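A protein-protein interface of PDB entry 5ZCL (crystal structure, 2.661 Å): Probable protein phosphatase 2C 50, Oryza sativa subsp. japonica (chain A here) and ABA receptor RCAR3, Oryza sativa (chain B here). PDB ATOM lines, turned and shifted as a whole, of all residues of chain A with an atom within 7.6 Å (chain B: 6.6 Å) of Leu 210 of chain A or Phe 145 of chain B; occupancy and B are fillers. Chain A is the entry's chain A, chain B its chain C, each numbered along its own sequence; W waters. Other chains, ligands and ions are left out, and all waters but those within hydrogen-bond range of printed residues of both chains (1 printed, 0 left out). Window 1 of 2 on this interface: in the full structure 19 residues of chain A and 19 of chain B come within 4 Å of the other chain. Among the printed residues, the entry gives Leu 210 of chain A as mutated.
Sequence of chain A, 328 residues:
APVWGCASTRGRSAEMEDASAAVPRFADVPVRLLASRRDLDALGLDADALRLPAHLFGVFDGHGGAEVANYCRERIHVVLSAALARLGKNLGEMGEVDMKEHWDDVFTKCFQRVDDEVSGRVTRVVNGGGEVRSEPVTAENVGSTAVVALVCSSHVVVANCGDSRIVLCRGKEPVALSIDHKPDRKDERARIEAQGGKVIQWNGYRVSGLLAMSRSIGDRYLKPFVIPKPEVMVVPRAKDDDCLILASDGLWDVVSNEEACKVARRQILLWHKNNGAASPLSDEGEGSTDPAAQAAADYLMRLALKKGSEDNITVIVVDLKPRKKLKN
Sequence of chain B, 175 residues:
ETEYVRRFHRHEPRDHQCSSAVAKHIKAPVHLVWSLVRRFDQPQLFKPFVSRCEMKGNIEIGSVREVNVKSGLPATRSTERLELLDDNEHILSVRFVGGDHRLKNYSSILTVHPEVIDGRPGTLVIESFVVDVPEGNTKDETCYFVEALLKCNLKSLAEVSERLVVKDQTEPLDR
The backbone carbonyl oxygen of Pro 74 of chain B lies within hydrogen-bond range of the side-chain amide nitrogen of Asn 203 of chain A, 3.1 Å away.
The side-chain amino group (NZ) of Lys 198 of chain A lies within salt-bridge range of the side-chain carboxylate (OD2) of Asp 140 of chain B.
N of Arg 206 of chain A sits at hydrogen-bond distance from O of Ile 200 of chain A (2.8 Å).
The backbone carbonyl oxygen of Leu 210 of chain A lies within hydrogen-bond range of the guanidinium group of Arg 206 of chain A (3.2 Å).
O of Lys 198 of chain A sits at hydrogen-bond distance from N of Ser 208 of chain A (2.8 Å).
NE of Arg 206 of chain A sits at hydrogen-bond distance from O of Trp 202 of chain A (3.0 Å).
The backbone carbonyl oxygen (O) of Asn 203 of chain A is in hydrogen-bond range of the guanidinium group (NH2) of Arg 206 of chain A (3.0 Å).
Of the 16 printed residues of chain B, 11 touch a printed residue of chain A.
Hydrophobic or aromatic side chains of chain B that line the printed part of chain A: Phe 49, Pro 74, Leu 103, Tyr 144, Phe 145 and Leu 149.
Printed residues of chain A that touch a printed residue of chain B: Lys 198, Ile 200, Trp 202, Asn 203, Arg 206, Ser 208, Gly 209, Leu 210, Leu 211 and Tyr 221.
Hydrophobic or aromatic side chains of chain A within 4 Å of the printed part of chain B: Ile 200, Trp 202, Leu 210, Leu 211 and Tyr 221.
Among the printed residues, Asp or Glu carboxylates within 4 Å of a Lys or Arg side-chain nitrogen of the other chain: Lys 198 of chain A with Asp 140 of chain B (3.3 Å).
Among the printed residues, pairs that only touch across the chains: Gly 209 of chain A with Phe 145 of chain B (3.1 Å), Gly 209 of chain A with Pro 74 of chain B (3.2 Å), Leu 210 of chain A with Phe 145 of chain B (3.5 Å), Leu 210 of chain A with Gly 72 of chain B (3.5 Å), Ser 208 of chain A with Tyr 144 of chain B (3.5 Å), Tyr 221 of chain A with Phe 49 of chain B (3.6 Å), Arg 206 of chain A with Pro 74 of chain B (3.6 Å), Leu 210 of chain A with Leu 149 of chain B (3.6 Å), Trp 202 of chain A with Pro 74 of chain B (3.7 Å), Arg 206 of chain A with Leu 73 of chain B (3.7 Å), Ile 200 of chain A with Glu 141 of chain B (3.8 Å), Trp 202 of chain A with Phe 145 of chain B (3.8 Å), Lys 198 of chain A with Tyr 144 of chain B (3.8 Å), Ser 208 of chain A with Phe 145 of chain B (3.8 Å), Leu 210 of chain A with Pro 74 of chain B (3.9 Å), Trp 202 of chain A with Leu 103 of chain B (3.9 Å), Trp 202 of chain A with Thr 142 of chain B (3.9 Å) and Leu 211 of chain A with Gly 72 of chain B (3.96 Å).
Water W1 lies within hydrogen-bond range of OG of Ser 208 of chain A, N of Lys 198 of chain A and OH of Tyr 144 of chain B.
Gly 204 of chain A touches none of the printed residues of chain B.
Leu 210 of chain A touches just these residues of chain B: Gly 72 (3.5 Å), Pro 74 (3.9 Å), Phe 145 (3.5 Å) and Leu 149 (3.6 Å).
Printed residues of chain A within 4 Å of Phe 49 of chain B: Tyr 221.
Of the printed residues of chain A, Leu 103 of chain B touches Trp 202 (3.9 Å).
The nearest residue of chain A that does not touch Phe 145 of chain B is Ile 200 of chain A (4.6 Å).
The nearest printed residue of chain A that does not touch Pro 74 of chain B is Leu 211 of chain A (5.9 Å).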
ATOM      1  N   LYS A 198     -23.930  -0.601  12.857  1.00  0.00           N
ATOM      2  CA  LYS A 198     -25.061   0.043  12.219  1.00  0.00           C
ATOM      3  C   LYS A 198     -26.201  -0.951  12.068  1.00  0.00           C
ATOM      4  O   LYS A 198     -25.986  -2.115  11.724  1.00  0.00           O
ATOM      5  CB  LYS A 198     -24.690   0.630  10.843  1.00  0.00           C
ATOM      6  CG  LYS A 198     -23.667   1.741  10.922  1.00  0.00           C
ATOM      7  CD  LYS A 198     -23.428   2.381   9.577  1.00  0.00           C
ATOM      8  CE  LYS A 198     -22.430   3.526   9.705  1.00  0.00           C
ATOM      9  NZ  LYS A 198     -22.994   4.678  10.459  1.00  0.00           N
ATOM     10  N   ILE A 200     -29.159  -1.053   9.618  1.00  0.00           N
ATOM     11  CA  ILE A 200     -29.534  -0.410   8.363  1.00  0.00           C
ATOM     12  C   ILE A 200     -30.851  -0.993   7.870  1.00  0.00           C
ATOM     13  O   ILE A 200     -31.091  -2.197   7.995  1.00  0.00           O
ATOM     14  CB  ILE A 200     -28.433  -0.581   7.300  1.00  0.00           C
ATOM     15  CG1 ILE A 200     -27.105  -0.044   7.833  1.00  0.00           C
ATOM     16  CG2 ILE A 200     -28.848   0.072   5.997  1.00  0.00           C
ATOM     17  CD1 ILE A 200     -25.902  -0.451   7.013  1.00  0.00           C
ATOM     18  N   TRP A 202     -32.611  -2.165   4.941  1.00  0.00           N
ATOM     19  CA  TRP A 202     -32.131  -2.670   3.657  1.00  0.00           C
ATOM     20  C   TRP A 202     -32.934  -3.938   3.353  1.00  0.00           C
ATOM     21  O   TRP A 202     -32.501  -5.070   3.609  1.00  0.00           O
ATOM     22  CB  TRP A 202     -30.633  -2.952   3.716  1.00  0.00           C
ATOM     23  CG  TRP A 202     -29.979  -3.024   2.393  1.00  0.00           C
ATOM     24  CD1 TRP A 202     -30.056  -4.040   1.497  1.00  0.00           C
ATOM     25  CD2 TRP A 202     -29.113  -2.043   1.816  1.00  0.00           C
ATOM     26  NE1 TRP A 202     -29.294  -3.757   0.393  1.00  0.00           N
ATOM     27  CE2 TRP A 202     -28.706  -2.534   0.563  1.00  0.00           C
ATOM     28  CE3 TRP A 202     -28.643  -0.797   2.238  1.00  0.00           C
ATOM     29  CZ2 TRP A 202     -27.855  -1.821  -0.278  1.00  0.00           C
ATOM     30  CZ3 TRP A 202     -27.798  -0.092   1.403  1.00  0.00           C
ATOM     31  CH2 TRP A 202     -27.412  -0.606   0.160  1.00  0.00           C
ATOM     32  N   ASN A 203     -34.161  -3.745   2.864  1.00  0.00           N
ATOM     33  CA  ASN A 203     -35.110  -4.850   2.730  1.00  0.00           C
ATOM     34  C   ASN A 203     -35.369  -5.474   4.107  1.00  0.00           C
ATOM     35  O   ASN A 203     -35.227  -6.682   4.310  1.00  0.00           O
ATOM     36  CB  ASN A 203     -34.604  -5.890   1.723  1.00  0.00           C
ATOM     37  CG  ASN A 203     -35.629  -6.976   1.421  1.00  0.00           C
ATOM     38  OD1 ASN A 203     -36.840  -6.759   1.511  1.00  0.00           O
ATOM     39  ND2 ASN A 203     -35.142  -8.157   1.057  1.00  0.00           N
ATOM     40  N   GLY A 204     -35.726  -4.627   5.063  1.00  0.00           N
ATOM     41  CA  GLY A 204     -35.869  -4.998   6.456  1.00  0.00           C
ATOM     42  C   GLY A 204     -34.701  -4.487   7.276  1.00  0.00           C
ATOM     43  O   GLY A 204     -33.599  -4.263   6.766  1.00  0.00           O
ATOM     44  N   TYR A 205     -34.941  -4.260   8.563  1.00  0.00           N
ATOM     45  CA  TYR A 205     -33.863  -3.775   9.420  1.00  0.00           C
ATOM     46  C   TYR A 205     -32.834  -4.879   9.651  1.00  0.00           C
ATOM     47  O   TYR A 205     -33.172  -5.965  10.130  1.00  0.00           O
ATOM     48  CB  TYR A 205     -34.414  -3.231  10.738  1.00  0.00           C
ATOM     49  CG  TYR A 205     -35.020  -1.867  10.549  1.00  0.00           C
ATOM     50  CD1 TYR A 205     -34.211  -0.734  10.491  1.00  0.00           C
ATOM     51  CD2 TYR A 205     -36.393  -1.705  10.398  1.00  0.00           C
ATOM     52  CE1 TYR A 205     -34.748   0.519  10.291  1.00  0.00           C
ATOM     53  CE2 TYR A 205     -36.943  -0.451  10.200  1.00  0.00           C
ATOM     54  CZ  TYR A 205     -36.116   0.657  10.149  1.00  0.00           C
ATOM     55  OH  TYR A 205     -36.660   1.907   9.952  1.00  0.00           O
ATOM     56  N   ARG A 206     -31.580  -4.609   9.300  1.00  0.00           N
ATOM     57  CA  ARG A 206     -30.538  -5.621   9.296  1.00  0.00           C
ATOM     58  C   ARG A 206     -29.264  -5.094   9.940  1.00  0.00           C
ATOM     59  O   ARG A 206     -28.927  -3.913   9.826  1.00  0.00           O
ATOM     60  CB  ARG A 206     -30.238  -6.091   7.864  1.00  0.00           C
ATOM     61  CG  ARG A 206     -31.463  -6.589   7.129  1.00  0.00           C
ATOM     62  CD  ARG A 206     -31.125  -7.143   5.763  1.00  0.00           C
ATOM     63  NE  ARG A 206     -32.333  -7.639   5.109  1.00  0.00           N
ATOM     64  CZ  ARG A 206     -32.666  -8.924   5.008  1.00  0.00           C
ATOM     65  NH1 ARG A 206     -31.885  -9.864   5.505  1.00  0.00           N
ATOM     66  NH2 ARG A 206     -33.789  -9.277   4.401  1.00  0.00           N
ATOM     67  N   VAL A 207     -28.544  -6.000  10.600  1.00  0.00           N
ATOM     68  CA  VAL A 207     -27.249  -5.662  11.173  1.00  0.00           C
ATOM     69  C   VAL A 207     -26.261  -5.479  10.033  1.00  0.00           C
ATOM     70  O   VAL A 207     -26.086  -6.372   9.194  1.00  0.00           O
ATOM     71  CB  VAL A 207     -26.772  -6.748  12.142  1.00  0.00           C
ATOM     72  CG1 VAL A 207     -25.366  -6.430  12.611  1.00  0.00           C
ATOM     73  CG2 VAL A 207     -27.718  -6.862  13.305  1.00  0.00           C
ATOM     74  N   SER A 208     -25.632  -4.310   9.977  1.00  0.00           N
ATOM     75  CA  SER A 208     -24.744  -3.962   8.876  1.00  0.00           C
ATOM     76  C   SER A 208     -25.454  -4.035   7.535  1.00  0.00           C
ATOM     77  O   SER A 208     -24.809  -4.124   6.491  1.00  0.00           O
ATOM     78  CB  SER A 208     -23.510  -4.870   8.858  1.00  0.00           C
ATOM     79  OG  SER A 208     -22.901  -4.928  10.134  1.00  0.00           O
ATOM     80  N   GLY A 209     -26.781  -4.002   7.548  1.00  0.00           N
ATOM     81  CA  GLY A 209     -27.561  -4.192   6.347  1.00  0.00           C
ATOM     82  C   GLY A 209     -27.594  -5.606   5.819  1.00  0.00           C
ATOM     83  O   GLY A 209     -28.089  -5.815   4.710  1.00  0.00           O
ATOM     84  N   LEU A 210     -27.157  -6.596   6.601  1.00  0.00           N
ATOM     85  CA  LEU A 210     -27.025  -7.966   6.112  1.00  0.00           C
ATOM     86  C   LEU A 210     -27.945  -8.941   6.833  1.00  0.00           C
ATOM     87  O   LEU A 210     -28.820  -9.534   6.193  1.00  0.00           O
ATOM     88  CB  LEU A 210     -25.569  -8.436   6.238  1.00  0.00           C
ATOM     89  CG  LEU A 210     -24.564  -7.665   5.395  1.00  0.00           C
ATOM     90  CD1 LEU A 210     -23.155  -8.081   5.735  1.00  0.00           C
ATOM     91  CD2 LEU A 210     -24.871  -7.912   3.927  1.00  0.00           C
ATOM     92  N   LEU A 211     -27.763  -9.139   8.140  1.00  0.00           N
ATOM     93  CA  LEU A 211     -28.488 -10.158   8.890  1.00  0.00           C
ATOM     94  C   LEU A 211     -29.748  -9.570   9.515  1.00  0.00           C
ATOM     95  O   LEU A 211     -29.694  -8.517  10.156  1.00  0.00           O
ATOM     96  CB  LEU A 211     -27.589 -10.752   9.969  1.00  0.00           C
ATOM     97  CG  LEU A 211     -28.022 -12.097  10.523  1.00  0.00           C
ATOM     98  CD1 LEU A 211     -28.137 -13.107   9.395  1.00  0.00           C
ATOM     99  CD2 LEU A 211     -27.035 -12.564  11.572  1.00  0.00           C
ATOM    100  N   ALA A 212     -30.883 -10.261   9.337  1.00  0.00           N
ATOM    101  CA  ALA A 212     -32.172  -9.794   9.839  1.00  0.00           C
ATOM    102  C   ALA A 212     -32.436 -10.196  11.288  1.00  0.00           C
ATOM    103  O   ALA A 212     -33.603 -10.292  11.687  1.00  0.00           O
ATOM    104  CB  ALA A 212     -33.307 -10.293   8.944  1.00  0.00           C
ATOM    105  N   MET A 213     -31.392 -10.410  12.089  1.00  0.00           N
ATOM    106  CA  MET A 213     -31.554 -10.656  13.517  1.00  0.00           C
ATOM    107  C   MET A 213     -30.312 -10.141  14.225  1.00  0.00           C
ATOM    108  O   MET A 213     -29.253  -9.986  13.617  1.00  0.00           O
ATOM    109  CB  MET A 213     -31.775 -12.141  13.832  1.00  0.00           C
ATOM    110  CG  MET A 213     -30.547 -12.996  13.583  1.00  0.00           C
ATOM    111  SD  MET A 213     -30.899 -14.756  13.460  1.00  0.00           S
ATOM    112  CE  MET A 213     -32.104 -14.782  12.135  1.00  0.00           C
ATOM    113  N   TYR A 221     -18.278 -13.333  11.360  1.00  0.00           N
ATOM    114  CA  TYR A 221     -17.920 -12.168  10.560  1.00  0.00           C
ATOM    115  C   TYR A 221     -18.732 -10.930  10.915  1.00  0.00           C
ATOM    116  O   TYR A 221     -18.387  -9.839  10.453  1.00  0.00           O
ATOM    117  CB  TYR A 221     -18.080 -12.478   9.065  1.00  0.00           C
ATOM    118  CG  TYR A 221     -19.447 -12.203   8.458  1.00  0.00           C
ATOM    119  CD1 TYR A 221     -20.554 -13.011   8.754  1.00  0.00           C
ATOM    120  CD2 TYR A 221     -19.625 -11.159   7.559  1.00  0.00           C
ATOM    121  CE1 TYR A 221     -21.803 -12.767   8.181  1.00  0.00           C
ATOM    122  CE2 TYR A 221     -20.871 -10.905   6.985  1.00  0.00           C
ATOM    123  CZ  TYR A 221     -21.946 -11.708   7.297  1.00  0.00           C
ATOM    124  OH  TYR A 221     -23.158 -11.443   6.715  1.00  0.00           O
ATOM    125  N   LEU A 222     -19.784 -11.066  11.724  1.00  0.00           N
ATOM    126  CA  LEU A 222     -20.585  -9.937  12.182  1.00  0.00           C
ATOM    127  C   LEU A 222     -20.364  -9.637  13.653  1.00  0.00           C
ATOM    128  O   LEU A 222     -21.186  -8.950  14.270  1.00  0.00           O
ATOM    129  CB  LEU A 222     -22.070 -10.177  11.921  1.00  0.00           C
ATOM    130  CG  LEU A 222     -22.497 -10.008  10.469  1.00  0.00           C
ATOM    131  CD1 LEU A 222     -23.970 -10.311  10.347  1.00  0.00           C
ATOM    132  CD2 LEU A 222     -22.202  -8.593  10.022  1.00  0.00           C
ATOM    133  N   PHE B  49     -20.269 -15.976   0.043  1.00  0.00           N
ATOM    134  CA  PHE B  49     -21.697 -15.736  -0.070  1.00  0.00           C
ATOM    135  C   PHE B  49     -22.309 -16.325  -1.330  1.00  0.00           C
ATOM    136  O   PHE B  49     -23.541 -16.346  -1.448  1.00  0.00           O
ATOM    137  CB  PHE B  49     -21.968 -14.234  -0.040  1.00  0.00           C
ATOM    138  CG  PHE B  49     -21.731 -13.612   1.296  1.00  0.00           C
ATOM    139  CD1 PHE B  49     -22.649 -13.778   2.316  1.00  0.00           C
ATOM    140  CD2 PHE B  49     -20.593 -12.854   1.530  1.00  0.00           C
ATOM    141  CE1 PHE B  49     -22.433 -13.215   3.554  1.00  0.00           C
ATOM    142  CE2 PHE B  49     -20.372 -12.284   2.763  1.00  0.00           C
ATOM    143  CZ  PHE B  49     -21.295 -12.464   3.780  1.00  0.00           C
ATOM    144  N   GLY B  72     -29.819 -15.839   4.298  1.00  0.00           N
ATOM    145  CA  GLY B  72     -29.390 -14.879   5.299  1.00  0.00           C
ATOM    146  C   GLY B  72     -28.886 -13.558   4.765  1.00  0.00           C
ATOM    147  O   GLY B  72     -28.101 -12.889   5.443  1.00  0.00           O
ATOM    148  N   LEU B  73     -29.297 -13.169   3.566  1.00  0.00           N
ATOM    149  CA  LEU B  73     -28.896 -11.924   2.923  1.00  0.00           C
ATOM    150  C   LEU B  73     -30.138 -11.195   2.454  1.00  0.00           C
ATOM    151  O   LEU B  73     -31.231 -11.764   2.395  1.00  0.00           O
ATOM    152  CB  LEU B  73     -27.959 -12.176   1.729  1.00  0.00           C
ATOM    153  CG  LEU B  73     -26.548 -12.720   1.963  1.00  0.00           C
ATOM    154  CD1 LEU B  73     -25.989 -13.222   0.650  1.00  0.00           C
ATOM    155  CD2 LEU B  73     -25.647 -11.644   2.525  1.00  0.00           C
ATOM    156  N   PRO B  74     -30.005  -9.914   2.112  1.00  0.00           N
ATOM    157  CA  PRO B  74     -31.146  -9.150   1.599  1.00  0.00           C
ATOM    158  C   PRO B  74     -31.488  -9.445   0.145  1.00  0.00           C
ATOM    159  O   PRO B  74     -32.448  -8.865  -0.372  1.00  0.00           O
ATOM    160  CB  PRO B  74     -30.686  -7.689   1.764  1.00  0.00           C
ATOM    161  CG  PRO B  74     -29.458  -7.739   2.611  1.00  0.00           C
ATOM    162  CD  PRO B  74     -28.833  -9.068   2.361  1.00  0.00           C
ATOM    163  N   LEU B 103     -28.246  -2.907  -5.180  1.00  0.00           N
ATOM    164  CA  LEU B 103     -27.011  -2.266  -5.645  1.00  0.00           C
ATOM    165  C   LEU B 103     -27.105  -1.969  -7.144  1.00  0.00           C
ATOM    166  O   LEU B 103     -26.574  -2.697  -7.986  1.00  0.00           O
ATOM    167  CB  LEU B 103     -25.808  -3.143  -5.320  1.00  0.00           C
ATOM    168  CG  LEU B 103     -25.541  -3.301  -3.831  1.00  0.00           C
ATOM    169  CD1 LEU B 103     -24.318  -4.164  -3.607  1.00  0.00           C
ATOM    170  CD2 LEU B 103     -25.348  -1.939  -3.216  1.00  0.00           C
ATOM    171  N   ASP B 140     -23.202   6.803   3.751  1.00  0.00           N
ATOM    172  CA  ASP B 140     -22.443   6.059   4.752  1.00  0.00           C
ATOM    173  C   ASP B 140     -22.978   4.637   4.911  1.00  0.00           C
ATOM    174  O   ASP B 140     -22.205   3.671   4.920  1.00  0.00           O
ATOM    175  CB  ASP B 140     -22.477   6.801   6.088  1.00  0.00           C
ATOM    176  CG  ASP B 140     -21.415   6.312   7.060  1.00  0.00           C
ATOM    177  OD1 ASP B 140     -20.520   5.542   6.641  1.00  0.00           O
ATOM    178  OD2 ASP B 140     -21.484   6.694   8.251  1.00  0.00           O
ATOM    179  N   GLU B 141     -24.299   4.487   5.024  1.00  0.00           N
ATOM    180  CA  GLU B 141     -24.887   3.156   5.134  1.00  0.00           C
ATOM    181  C   GLU B 141     -24.491   2.286   3.946  1.00  0.00           C
ATOM    182  O   GLU B 141     -24.108   1.121   4.110  1.00  0.00           O
ATOM    183  CB  GLU B 141     -26.409   3.263   5.232  1.00  0.00           C
ATOM    184  CG  GLU B 141     -26.921   3.799   6.551  1.00  0.00           C
ATOM    185  CD  GLU B 141     -28.431   3.948   6.561  1.00  0.00           C
ATOM    186  OE1 GLU B 141     -29.006   4.335   5.511  1.00  0.00           O
ATOM    187  OE2 GLU B 141     -29.038   3.697   7.627  1.00  0.00           O
ATOM    188  N   THR B 142     -24.595   2.831   2.735  1.00  0.00           N
ATOM    189  CA  THR B 142     -24.269   2.045   1.550  1.00  0.00           C
ATOM    190  C   THR B 142     -22.811   1.600   1.564  1.00  0.00           C
ATOM    191  O   THR B 142     -22.502   0.431   1.311  1.00  0.00           O
ATOM    192  CB  THR B 142     -24.575   2.849   0.291  1.00  0.00           C
ATOM    193  OG1 THR B 142     -25.971   3.182   0.265  1.00  0.00           O
ATOM    194  CG2 THR B 142     -24.198   2.053  -0.947  1.00  0.00           C
ATOM    195  N   CYS B 143     -21.897   2.513   1.883  1.00  0.00           N
ATOM    196  CA  CYS B 143     -20.493   2.130   1.931  1.00  0.00           C
ATOM    197  C   CYS B 143     -20.252   1.084   3.009  1.00  0.00           C
ATOM    198  O   CYS B 143     -19.456   0.159   2.815  1.00  0.00           O
ATOM    199  CB  CYS B 143     -19.618   3.364   2.155  1.00  0.00           C
ATOM    200  SG  CYS B 143     -19.486   4.402   0.679  1.00  0.00           S
ATOM    201  N   TYR B 144     -20.946   1.200   4.146  1.00  0.00           N
ATOM    202  CA  TYR B 144     -20.784   0.220   5.216  1.00  0.00           C
ATOM    203  C   TYR B 144     -21.233  -1.159   4.755  1.00  0.00           C
ATOM    204  O   TYR B 144     -20.526  -2.158   4.946  1.00  0.00           O
ATOM    205  CB  TYR B 144     -21.577   0.663   6.451  1.00  0.00           C
ATOM    206  CG  TYR B 144     -21.177  -0.028   7.738  1.00  0.00           C
ATOM    207  CD1 TYR B 144     -20.163   0.478   8.529  1.00  0.00           C
ATOM    208  CD2 TYR B 144     -21.823  -1.177   8.165  1.00  0.00           C
ATOM    209  CE1 TYR B 144     -19.787  -0.140   9.694  1.00  0.00           C
ATOM    210  CE2 TYR B 144     -21.460  -1.809   9.345  1.00  0.00           C
ATOM    211  CZ  TYR B 144     -20.438  -1.283  10.107  1.00  0.00           C
ATOM    212  OH  TYR B 144     -20.061  -1.901  11.285  1.00  0.00           O
ATOM    213  N   PHE B 145     -22.399  -1.219   4.108  1.00  0.00           N
ATOM    214  CA  PHE B 145     -22.928  -2.475   3.589  1.00  0.00           C
ATOM    215  C   PHE B 145     -21.930  -3.158   2.661  1.00  0.00           C
ATOM    216  O   PHE B 145     -21.662  -4.360   2.793  1.00  0.00           O
ATOM    217  CB  PHE B 145     -24.238  -2.186   2.864  1.00  0.00           C
ATOM    218  CG  PHE B 145     -24.840  -3.364   2.171  1.00  0.00           C
ATOM    219  CD1 PHE B 145     -24.532  -3.635   0.848  1.00  0.00           C
ATOM    220  CD2 PHE B 145     -25.747  -4.178   2.826  1.00  0.00           C
ATOM    221  CE1 PHE B 145     -25.096  -4.708   0.195  1.00  0.00           C
ATOM    222  CE2 PHE B 145     -26.322  -5.250   2.176  1.00  0.00           C
ATOM    223  CZ  PHE B 145     -25.999  -5.516   0.856  1.00  0.00           C
ATOM    224  N   VAL B 146     -21.352  -2.399   1.728  1.00  0.00           N
ATOM    225  CA  VAL B 146     -20.464  -2.999   0.742  1.00  0.00           C
ATOM    226  C   VAL B 146     -19.128  -3.366   1.377  1.00  0.00           C
ATOM    227  O   VAL B 146     -18.593  -4.457   1.139  1.00  0.00           O
ATOM    228  CB  VAL B 146     -20.293  -2.050  -0.457  1.00  0.00           C
ATOM    229  CG1 VAL B 146     -19.273  -2.594  -1.438  1.00  0.00           C
ATOM    230  CG2 VAL B 146     -21.629  -1.838  -1.154  1.00  0.00           C
ATOM    231  N   GLU B 147     -18.566  -2.468   2.189  1.00  0.00           N
ATOM    232  CA  GLU B 147     -17.258  -2.742   2.771  1.00  0.00           C
ATOM    233  C   GLU B 147     -17.307  -3.998   3.615  1.00  0.00           C
ATOM    234  O   GLU B 147     -16.354  -4.784   3.623  1.00  0.00           O
ATOM    235  CB  GLU B 147     -16.774  -1.561   3.613  1.00  0.00           C
ATOM    236  CG  GLU B 147     -16.372  -0.330   2.827  1.00  0.00           C
ATOM    237  CD  GLU B 147     -16.148   0.864   3.734  1.00  0.00           C
ATOM    238  OE1 GLU B 147     -16.029   0.651   4.962  1.00  0.00           O
ATOM    239  OE2 GLU B 147     -16.097   2.010   3.230  1.00  0.00           O
ATOM    240  N   ALA B 148     -18.421  -4.213   4.321  1.00  0.00           N
ATOM    241  CA  ALA B 148     -18.550  -5.418   5.139  1.00  0.00           C
ATOM    242  C   ALA B 148     -18.465  -6.669   4.276  1.00  0.00           C
ATOM    243  O   ALA B 148     -17.763  -7.623   4.624  1.00  0.00           O
ATOM    244  CB  ALA B 148     -19.858  -5.394   5.931  1.00  0.00           C
ATOM    245  N   LEU B 149     -19.167  -6.676   3.138  1.00  0.00           N
ATOM    246  CA  LEU B 149     -19.105  -7.821   2.234  1.00  0.00           C
ATOM    247  C   LEU B 149     -17.721  -7.963   1.602  1.00  0.00           C
ATOM    248  O   LEU B 149     -17.163  -9.065   1.561  1.00  0.00           O
ATOM    249  CB  LEU B 149     -20.182  -7.700   1.157  1.00  0.00           C
ATOM    250  CG  LEU B 149     -21.642  -7.767   1.609  1.00  0.00           C
ATOM    251  CD1 LEU B 149     -22.600  -7.450   0.467  1.00  0.00           C
ATOM    252  CD2 LEU B 149     -21.952  -9.140   2.178  1.00  0.00           C
ATOM    253  N   LEU B 150     -17.146  -6.859   1.106  1.00  0.00           N
ATOM    254  CA  LEU B 150     -15.834  -6.933   0.462  1.00  0.00           C
ATOM    255  C   LEU B 150     -14.739  -7.344   1.447  1.00  0.00           C
ATOM    256  O   LEU B 150     -13.885  -8.180   1.126  1.00  0.00           O
ATOM    257  CB  LEU B 150     -15.489  -5.595  -0.192  1.00  0.00           C
ATOM    258  CG  LEU B 150     -16.397  -5.076  -1.308  1.00  0.00           C
ATOM    259  CD1 LEU B 150     -15.781  -3.847  -1.943  1.00  0.00           C
ATOM    260  CD2 LEU B 150     -16.657  -6.139  -2.361  1.00  0.00           C
HETATM  261  O   HOH W   1     -23.027  -3.166  12.166  1.00  0.00           O
